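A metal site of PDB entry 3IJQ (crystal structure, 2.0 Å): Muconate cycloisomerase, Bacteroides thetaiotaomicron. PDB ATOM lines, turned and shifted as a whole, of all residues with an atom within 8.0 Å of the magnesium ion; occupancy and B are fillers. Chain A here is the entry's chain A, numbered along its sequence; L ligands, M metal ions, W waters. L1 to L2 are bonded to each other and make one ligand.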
ATOM      1  N   TYR A  49      18.958  11.265 -18.565  1.00  0.00           N
ATOM      2  CA  TYR A  49      20.368  11.009 -18.313  1.00  0.00           C
ATOM      3  C   TYR A  49      20.516   9.703 -17.552  1.00  0.00           C
ATOM      4  O   TYR A  49      21.564   9.429 -16.965  1.00  0.00           O
ATOM      5  CB  TYR A  49      20.977  12.174 -17.512  1.00  0.00           C
ATOM      6  CG  TYR A  49      20.437  12.326 -16.100  1.00  0.00           C
ATOM      7  CD1 TYR A  49      20.873  11.499 -15.075  1.00  0.00           C
ATOM      8  CD2 TYR A  49      19.481  13.295 -15.801  1.00  0.00           C
ATOM      9  CE1 TYR A  49      20.382  11.626 -13.782  1.00  0.00           C
ATOM     10  CE2 TYR A  49      18.977  13.434 -14.510  1.00  0.00           C
ATOM     11  CZ  TYR A  49      19.433  12.592 -13.512  1.00  0.00           C
ATOM     12  OH  TYR A  49      18.951  12.719 -12.225  1.00  0.00           O
ATOM     13  N   LYS A 153      17.074  19.749   1.448  1.00  0.00           N
ATOM     14  CA  LYS A 153      18.088  18.990   0.724  1.00  0.00           C
ATOM     15  C   LYS A 153      18.992  19.924  -0.068  1.00  0.00           C
ATOM     16  O   LYS A 153      18.522  20.886  -0.686  1.00  0.00           O
ATOM     17  CB  LYS A 153      17.422  18.000  -0.218  1.00  0.00           C
ATOM     18  CG  LYS A 153      18.389  17.220  -1.088  1.00  0.00           C
ATOM     19  CD  LYS A 153      17.651  16.232  -1.975  1.00  0.00           C
ATOM     20  CE  LYS A 153      18.609  15.426  -2.824  1.00  0.00           C
ATOM     21  NZ  LYS A 153      17.869  14.504  -3.726  1.00  0.00           N
ATOM     22  N   LYS A 155      22.383  19.750  -2.831  1.00  0.00           N
ATOM     23  CA  LYS A 155      23.352  18.988  -3.613  1.00  0.00           C
ATOM     24  C   LYS A 155      24.751  19.597  -3.500  1.00  0.00           C
ATOM     25  O   LYS A 155      25.049  20.605  -4.156  1.00  0.00           O
ATOM     26  CB  LYS A 155      22.928  18.928  -5.095  1.00  0.00           C
ATOM     27  CG  LYS A 155      21.670  18.116  -5.352  1.00  0.00           C
ATOM     28  CD  LYS A 155      20.415  18.993  -5.290  1.00  0.00           C
ATOM     29  CE  LYS A 155      20.148  19.671  -6.626  1.00  0.00           C
ATOM     30  NZ  LYS A 155      19.741  18.691  -7.680  1.00  0.00           N
ATOM     31  N   VAL A 178      22.470  16.505   2.709  1.00  0.00           N
ATOM     32  CA  VAL A 178      23.200  16.838   1.490  1.00  0.00           C
ATOM     33  C   VAL A 178      23.444  15.649   0.569  1.00  0.00           C
ATOM     34  O   VAL A 178      23.702  14.534   1.037  1.00  0.00           O
ATOM     35  CB  VAL A 178      24.584  17.509   1.810  1.00  0.00           C
ATOM     36  CG1 VAL A 178      24.392  18.641   2.815  1.00  0.00           C
ATOM     37  CG2 VAL A 178      25.557  16.475   2.354  1.00  0.00           C
ATOM     38  N   ASP A 179      23.346  15.888  -0.725  1.00  0.00           N
ATOM     39  CA  ASP A 179      23.576  14.842  -1.714  1.00  0.00           C
ATOM     40  C   ASP A 179      24.837  15.197  -2.494  1.00  0.00           C
ATOM     41  O   ASP A 179      24.786  16.038  -3.404  1.00  0.00           O
ATOM     42  CB  ASP A 179      22.384  14.745  -2.665  1.00  0.00           C
ATOM     43  CG  ASP A 179      22.400  13.476  -3.490  1.00  0.00           C
ATOM     44  OD1 ASP A 179      23.482  12.884  -3.640  1.00  0.00           O
ATOM     45  OD2 ASP A 179      21.318  13.073  -3.976  1.00  0.00           O
ATOM     46  N   ALA A 180      25.962  14.574  -2.140  1.00  0.00           N
ATOM     47  CA  ALA A 180      27.243  14.833  -2.794  1.00  0.00           C
ATOM     48  C   ALA A 180      27.352  14.329  -4.241  1.00  0.00           C
ATOM     49  O   ALA A 180      28.063  14.910  -5.052  1.00  0.00           O
ATOM     50  CB  ALA A 180      28.384  14.269  -1.954  1.00  0.00           C
ATOM     51  N   ASN A 181      26.643  13.242  -4.554  1.00  0.00           N
ATOM     52  CA  ASN A 181      26.664  12.668  -5.900  1.00  0.00           C
ATOM     53  C   ASN A 181      28.056  12.215  -6.320  1.00  0.00           C
ATOM     54  O   ASN A 181      28.493  12.501  -7.432  1.00  0.00           O
ATOM     55  CB  ASN A 181      26.149  13.686  -6.919  1.00  0.00           C
ATOM     56  CG  ASN A 181      24.733  14.152  -6.624  1.00  0.00           C
ATOM     57  OD1 ASN A 181      23.770  13.400  -6.795  1.00  0.00           O
ATOM     58  ND2 ASN A 181      24.602  15.391  -6.172  1.00  0.00           N
ATOM     59  N   GLU A 206      24.639  11.847   1.579  1.00  0.00           N
ATOM     60  CA  GLU A 206      24.253  10.900   0.547  1.00  0.00           C
ATOM     61  C   GLU A 206      25.288  10.755  -0.553  1.00  0.00           C
ATOM     62  O   GLU A 206      25.629  11.730  -1.220  1.00  0.00           O
ATOM     63  CB  GLU A 206      22.910  11.320  -0.076  1.00  0.00           C
ATOM     64  CG  GLU A 206      22.581  10.668  -1.422  1.00  0.00           C
ATOM     65  CD  GLU A 206      21.188  11.017  -1.918  1.00  0.00           C
ATOM     66  OE1 GLU A 206      20.873  10.723  -3.091  1.00  0.00           O
ATOM     67  OE2 GLU A 206      20.400  11.575  -1.123  1.00  0.00           O
ATOM     68  N   GLN A 207      25.774   9.533  -0.739  1.00  0.00           N
ATOM     69  CA  GLN A 207      26.768   9.217  -1.771  1.00  0.00           C
ATOM     70  C   GLN A 207      27.909  10.236  -1.802  1.00  0.00           C
ATOM     71  O   GLN A 207      28.043  11.003  -2.759  1.00  0.00           O
ATOM     72  CB  GLN A 207      26.086   9.148  -3.141  1.00  0.00           C
ATOM     73  CG  GLN A 207      26.901   8.441  -4.212  1.00  0.00           C
ATOM     74  CD  GLN A 207      27.192   7.000  -3.850  1.00  0.00           C
ATOM     75  OE1 GLN A 207      26.284   6.206  -3.600  1.00  0.00           O
ATOM     76  NE2 GLN A 207      28.482   6.636  -3.825  1.00  0.00           N
ATOM     77  N   PHE A 229      24.393   7.471   3.227  1.00  0.00           N
ATOM     78  CA  PHE A 229      23.474   6.686   2.411  1.00  0.00           C
ATOM     79  C   PHE A 229      23.976   6.508   0.989  1.00  0.00           C
ATOM     80  O   PHE A 229      24.556   7.421   0.415  1.00  0.00           O
ATOM     81  CB  PHE A 229      22.100   7.363   2.398  1.00  0.00           C
ATOM     82  CG  PHE A 229      21.320   7.186   3.670  1.00  0.00           C
ATOM     83  CD1 PHE A 229      20.435   6.116   3.823  1.00  0.00           C
ATOM     84  CD2 PHE A 229      21.471   8.082   4.727  1.00  0.00           C
ATOM     85  CE1 PHE A 229      19.722   5.945   5.011  1.00  0.00           C
ATOM     86  CE2 PHE A 229      20.772   7.909   5.917  1.00  0.00           C
ATOM     87  CZ  PHE A 229      19.891   6.842   6.058  1.00  0.00           C
ATOM     88  N   ALA A 230      23.740   5.337   0.424  1.00  0.00           N
ATOM     89  CA  ALA A 230      24.158   5.036  -0.938  1.00  0.00           C
ATOM     90  C   ALA A 230      23.032   5.267  -1.936  1.00  0.00           C
ATOM     91  O   ALA A 230      21.882   4.904  -1.677  1.00  0.00           O
ATOM     92  CB  ALA A 230      24.646   3.602  -1.023  1.00  0.00           C
ATOM     93  N   ASP A 231      23.365   5.857  -3.074  1.00  0.00           N
ATOM     94  CA  ASP A 231      22.369   6.117  -4.103  1.00  0.00           C
ATOM     95  C   ASP A 231      22.863   5.557  -5.444  1.00  0.00           C
ATOM     96  O   ASP A 231      22.274   4.626  -5.994  1.00  0.00           O
ATOM     97  CB  ASP A 231      22.124   7.620  -4.233  1.00  0.00           C
ATOM     98  CG  ASP A 231      21.069   7.960  -5.275  1.00  0.00           C
ATOM     99  OD1 ASP A 231      20.710   7.079  -6.087  1.00  0.00           O
ATOM    100  OD2 ASP A 231      20.604   9.117  -5.287  1.00  0.00           O
ATOM    101  N   GLU A 232      23.939   6.145  -5.950  1.00  0.00           N
ATOM    102  CA  GLU A 232      24.520   5.705  -7.222  1.00  0.00           C
ATOM    103  C   GLU A 232      25.190   4.347  -7.055  1.00  0.00           C
ATOM    104  O   GLU A 232      25.345   3.591  -8.020  1.00  0.00           O
ATOM    105  CB  GLU A 232      25.566   6.726  -7.711  1.00  0.00           C
ATOM    106  CG  GLU A 232      24.998   8.004  -8.321  1.00  0.00           C
ATOM    107  CD  GLU A 232      24.307   8.904  -7.312  1.00  0.00           C
ATOM    108  OE1 GLU A 232      24.827   9.058  -6.180  1.00  0.00           O
ATOM    109  OE2 GLU A 232      23.247   9.478  -7.658  1.00  0.00           O
ATOM    110  N   ASN A 251      19.486   4.172  -0.388  1.00  0.00           N
ATOM    111  CA  ASN A 251      18.405   5.004  -0.882  1.00  0.00           C
ATOM    112  C   ASN A 251      17.693   4.220  -1.963  1.00  0.00           C
ATOM    113  O   ASN A 251      18.327   3.711  -2.903  1.00  0.00           O
ATOM    114  CB  ASN A 251      18.963   6.305  -1.469  1.00  0.00           C
ATOM    115  CG  ASN A 251      17.908   7.121  -2.187  1.00  0.00           C
ATOM    116  OD1 ASN A 251      16.857   7.438  -1.624  1.00  0.00           O
ATOM    117  ND2 ASN A 251      18.177   7.458  -3.449  1.00  0.00           N
ATOM    118  N   LYS A 253      14.754   3.959  -5.009  1.00  0.00           N
ATOM    119  CA  LYS A 253      13.967   4.714  -5.973  1.00  0.00           C
ATOM    120  C   LYS A 253      13.240   3.711  -6.883  1.00  0.00           C
ATOM    121  O   LYS A 253      13.877   2.877  -7.530  1.00  0.00           O
ATOM    122  CB  LYS A 253      14.863   5.663  -6.779  1.00  0.00           C
ATOM    123  CG  LYS A 253      15.654   6.614  -5.886  1.00  0.00           C
ATOM    124  CD  LYS A 253      15.899   7.960  -6.553  1.00  0.00           C
ATOM    125  CE  LYS A 253      17.241   8.021  -7.265  1.00  0.00           C
ATOM    126  NZ  LYS A 253      18.378   8.374  -6.360  1.00  0.00           N
ATOM    127  N   LYS A 256      14.385   2.796 -10.324  1.00  0.00           N
ATOM    128  CA  LYS A 256      15.627   2.036 -10.475  1.00  0.00           C
ATOM    129  C   LYS A 256      15.527   0.563 -10.076  1.00  0.00           C
ATOM    130  O   LYS A 256      16.217  -0.284 -10.650  1.00  0.00           O
ATOM    131  CB  LYS A 256      16.762   2.656  -9.643  1.00  0.00           C
ATOM    132  CG  LYS A 256      17.079   4.113  -9.923  1.00  0.00           C
ATOM    133  CD  LYS A 256      18.549   4.429  -9.617  1.00  0.00           C
ATOM    134  CE  LYS A 256      18.982   3.993  -8.220  1.00  0.00           C
ATOM    135  NZ  LYS A 256      18.301   4.746  -7.129  1.00  0.00           N
ATOM    136  N   MET A 278      16.278   4.932   3.021  1.00  0.00           N
ATOM    137  CA  MET A 278      15.696   6.216   2.672  1.00  0.00           C
ATOM    138  C   MET A 278      15.085   5.975   1.305  1.00  0.00           C
ATOM    139  O   MET A 278      15.483   5.052   0.590  1.00  0.00           O
ATOM    140  CB  MET A 278      16.766   7.327   2.628  1.00  0.00           C
ATOM    141  CG  MET A 278      17.651   7.349   1.403  1.00  0.00           C
ATOM    142  SD  MET A 278      18.713   8.810   1.408  1.00  0.00           S
ATOM    143  CE  MET A 278      17.690   9.982   0.505  1.00  0.00           C
ATOM    144  N   GLY A 280      13.700   7.837  -2.395  1.00  0.00           N
ATOM    145  CA  GLY A 280      13.792   9.026  -3.212  1.00  0.00           C
ATOM    146  C   GLY A 280      12.880   8.907  -4.404  1.00  0.00           C
ATOM    147  O   GLY A 280      12.030   8.021  -4.454  1.00  0.00           O
ATOM    148  N   CYS A 281      13.078   9.776  -5.379  1.00  0.00           N
ATOM    149  CA  CYS A 281      12.237   9.762  -6.556  1.00  0.00           C
ATOM    150  C   CYS A 281      12.844  10.609  -7.644  1.00  0.00           C
ATOM    151  O   CYS A 281      13.841  11.293  -7.419  1.00  0.00           O
ATOM    152  CB  CYS A 281      10.875  10.371  -6.227  1.00  0.00           C
ATOM    153  SG  CYS A 281      10.987  12.145  -5.789  1.00  0.00           S
ATOM    154  N   MET A 282      12.238  10.555  -8.815  1.00  0.00           N
ATOM    155  CA  MET A 282      12.638  11.367  -9.949  1.00  0.00           C
ATOM    156  C   MET A 282      11.482  12.361 -10.004  1.00  0.00           C
ATOM    157  O   MET A 282      10.537  12.261  -9.223  1.00  0.00           O
ATOM    158  CB  MET A 282      12.625  10.553 -11.241  1.00  0.00           C
ATOM    159  CG  MET A 282      13.265   9.181 -11.168  1.00  0.00           C
ATOM    160  SD  MET A 282      15.053   9.235 -11.066  1.00  0.00           S
ATOM    161  CE  MET A 282      15.264   9.338  -9.364  1.00  0.00           C
ATOM    162  N   ASP A 303      12.893  11.678   0.327  1.00  0.00           N
ATOM    163  CA  ASP A 303      12.989  12.765  -0.618  1.00  0.00           C
ATOM    164  C   ASP A 303      11.879  12.435  -1.616  1.00  0.00           C
ATOM    165  O   ASP A 303      12.134  11.910  -2.701  1.00  0.00           O
ATOM    166  CB  ASP A 303      14.361  12.776  -1.304  1.00  0.00           C
ATOM    167  CG  ASP A 303      14.563  13.995  -2.188  1.00  0.00           C
ATOM    168  OD1 ASP A 303      14.333  15.119  -1.701  1.00  0.00           O
ATOM    169  OD2 ASP A 303      14.937  13.826  -3.365  1.00  0.00           O
HETATM  170  N1  LIG L   1      13.865  15.761  -5.001  1.00  0.00           N
HETATM  171  C1  LIG L   1      14.035  14.787  -6.088  1.00  0.00           C
HETATM  172  C2  LIG L   1      15.430  14.706  -6.744  1.00  0.00           C
HETATM  173  O1  LIG L   1      16.225  15.625  -6.688  1.00  0.00           O
HETATM  174  C3  LIG L   1      13.009  15.042  -7.172  1.00  0.00           C
HETATM  175  N1  LG2 L   2      15.682  13.551  -7.360  1.00  0.00           N
HETATM  176  C1  LG2 L   2      16.930  13.299  -8.114  1.00  0.00           C
HETATM  177  C2  LG2 L   2      17.848  12.288  -7.399  1.00  0.00           C
HETATM  178  O1  LG2 L   2      19.056  12.315  -7.698  1.00  0.00           O
HETATM  179  C3  LG2 L   2      16.567  12.821  -9.519  1.00  0.00           C
HETATM  180  C4  LG2 L   2      16.607  13.942 -10.540  1.00  0.00           C
HETATM  181  C5  LG2 L   2      15.679  13.772 -11.727  1.00  0.00           C
HETATM  182  O2  LG2 L   2      16.175  13.802 -12.867  1.00  0.00           O
HETATM  183  O3  LG2 L   2      14.461  13.615 -11.522  1.00  0.00           O
HETATM  184  O4  LG2 L   2      17.359  11.508  -6.563  1.00  0.00           O
HETATM  185 MG    MG M   1      20.592  11.165  -4.994  1.00  0.00          MG
HETATM  186  O   HOH W   1      22.527  10.849  -4.982  1.00  0.00           O
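OD2 of Asp 303 lies within salt-bridge range of N1 of LIG L1 (2.8 Å).
The side-chain amino group (NZ) of Lys 253 lies within salt-bridge range of an oxygen (O4) of LG2 L2.
OH of Tyr 49 is in hydrogen-bond range of O2 of LG2 L2, 3.0 Å away.
A nitrogen (N1) of LG2 L2 is in hydrogen-bond range of the backbone carbonyl oxygen (O) of Cys 281, 2.9 Å away.
The side-chain amino group (NZ) of Lys 253 lies within salt-bridge range of the side-chain carboxylate (OD1) of Asp 231.
The backbone NH (N) of Glu 206 is in hydrogen-bond range of the backbone carbonyl oxygen (O) of Val 178.
The side-chain amide nitrogen (ND2) of Asn 251 sits close to the side-chain carboxylate (OD2) of Asp 231.
The backbone NH (N) of Ala 180 sits at hydrogen-bond distance from the backbone carbonyl oxygen (O) of Glu 206.
The side-chain carboxylate (OD2) of Asp 179 sits close to the side-chain amino group (NZ) of Lys 153, at 3.7 Å.
The backbone carbonyl oxygen (O) of Asp 179 sits at hydrogen-bond distance from the side-chain amide nitrogen (ND2) of Asn 181 (2.8 Å).
The side-chain amino group of Lys 253 lies close to the side-chain amide nitrogen of Asn 251 (3.1 Å).
The backbone NH (N) of Asp 231 sits at hydrogen-bond distance from the side-chain amide oxygen (OE1) of Gln 207, 3.0 Å away.
Lys 253 touches the magnesium ion (NZ to MG, 3.8 Å).
Of the 21 residues printed, 4 come within 4 Å of the magnesium ion.
The nearest printed residue that does not touch the magnesium ion is Glu 232 (4.1 Å).
The magnesium ion is bound by water W1 (2.0 Å), the side-chain carboxylate (OE1) of Glu 206 (2.0 Å), the side-chain carboxylate (OD2) of Asp 231 (2.1 Å) and the side-chain carboxylate (OD2) of Asp 179 (2.3 Å).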
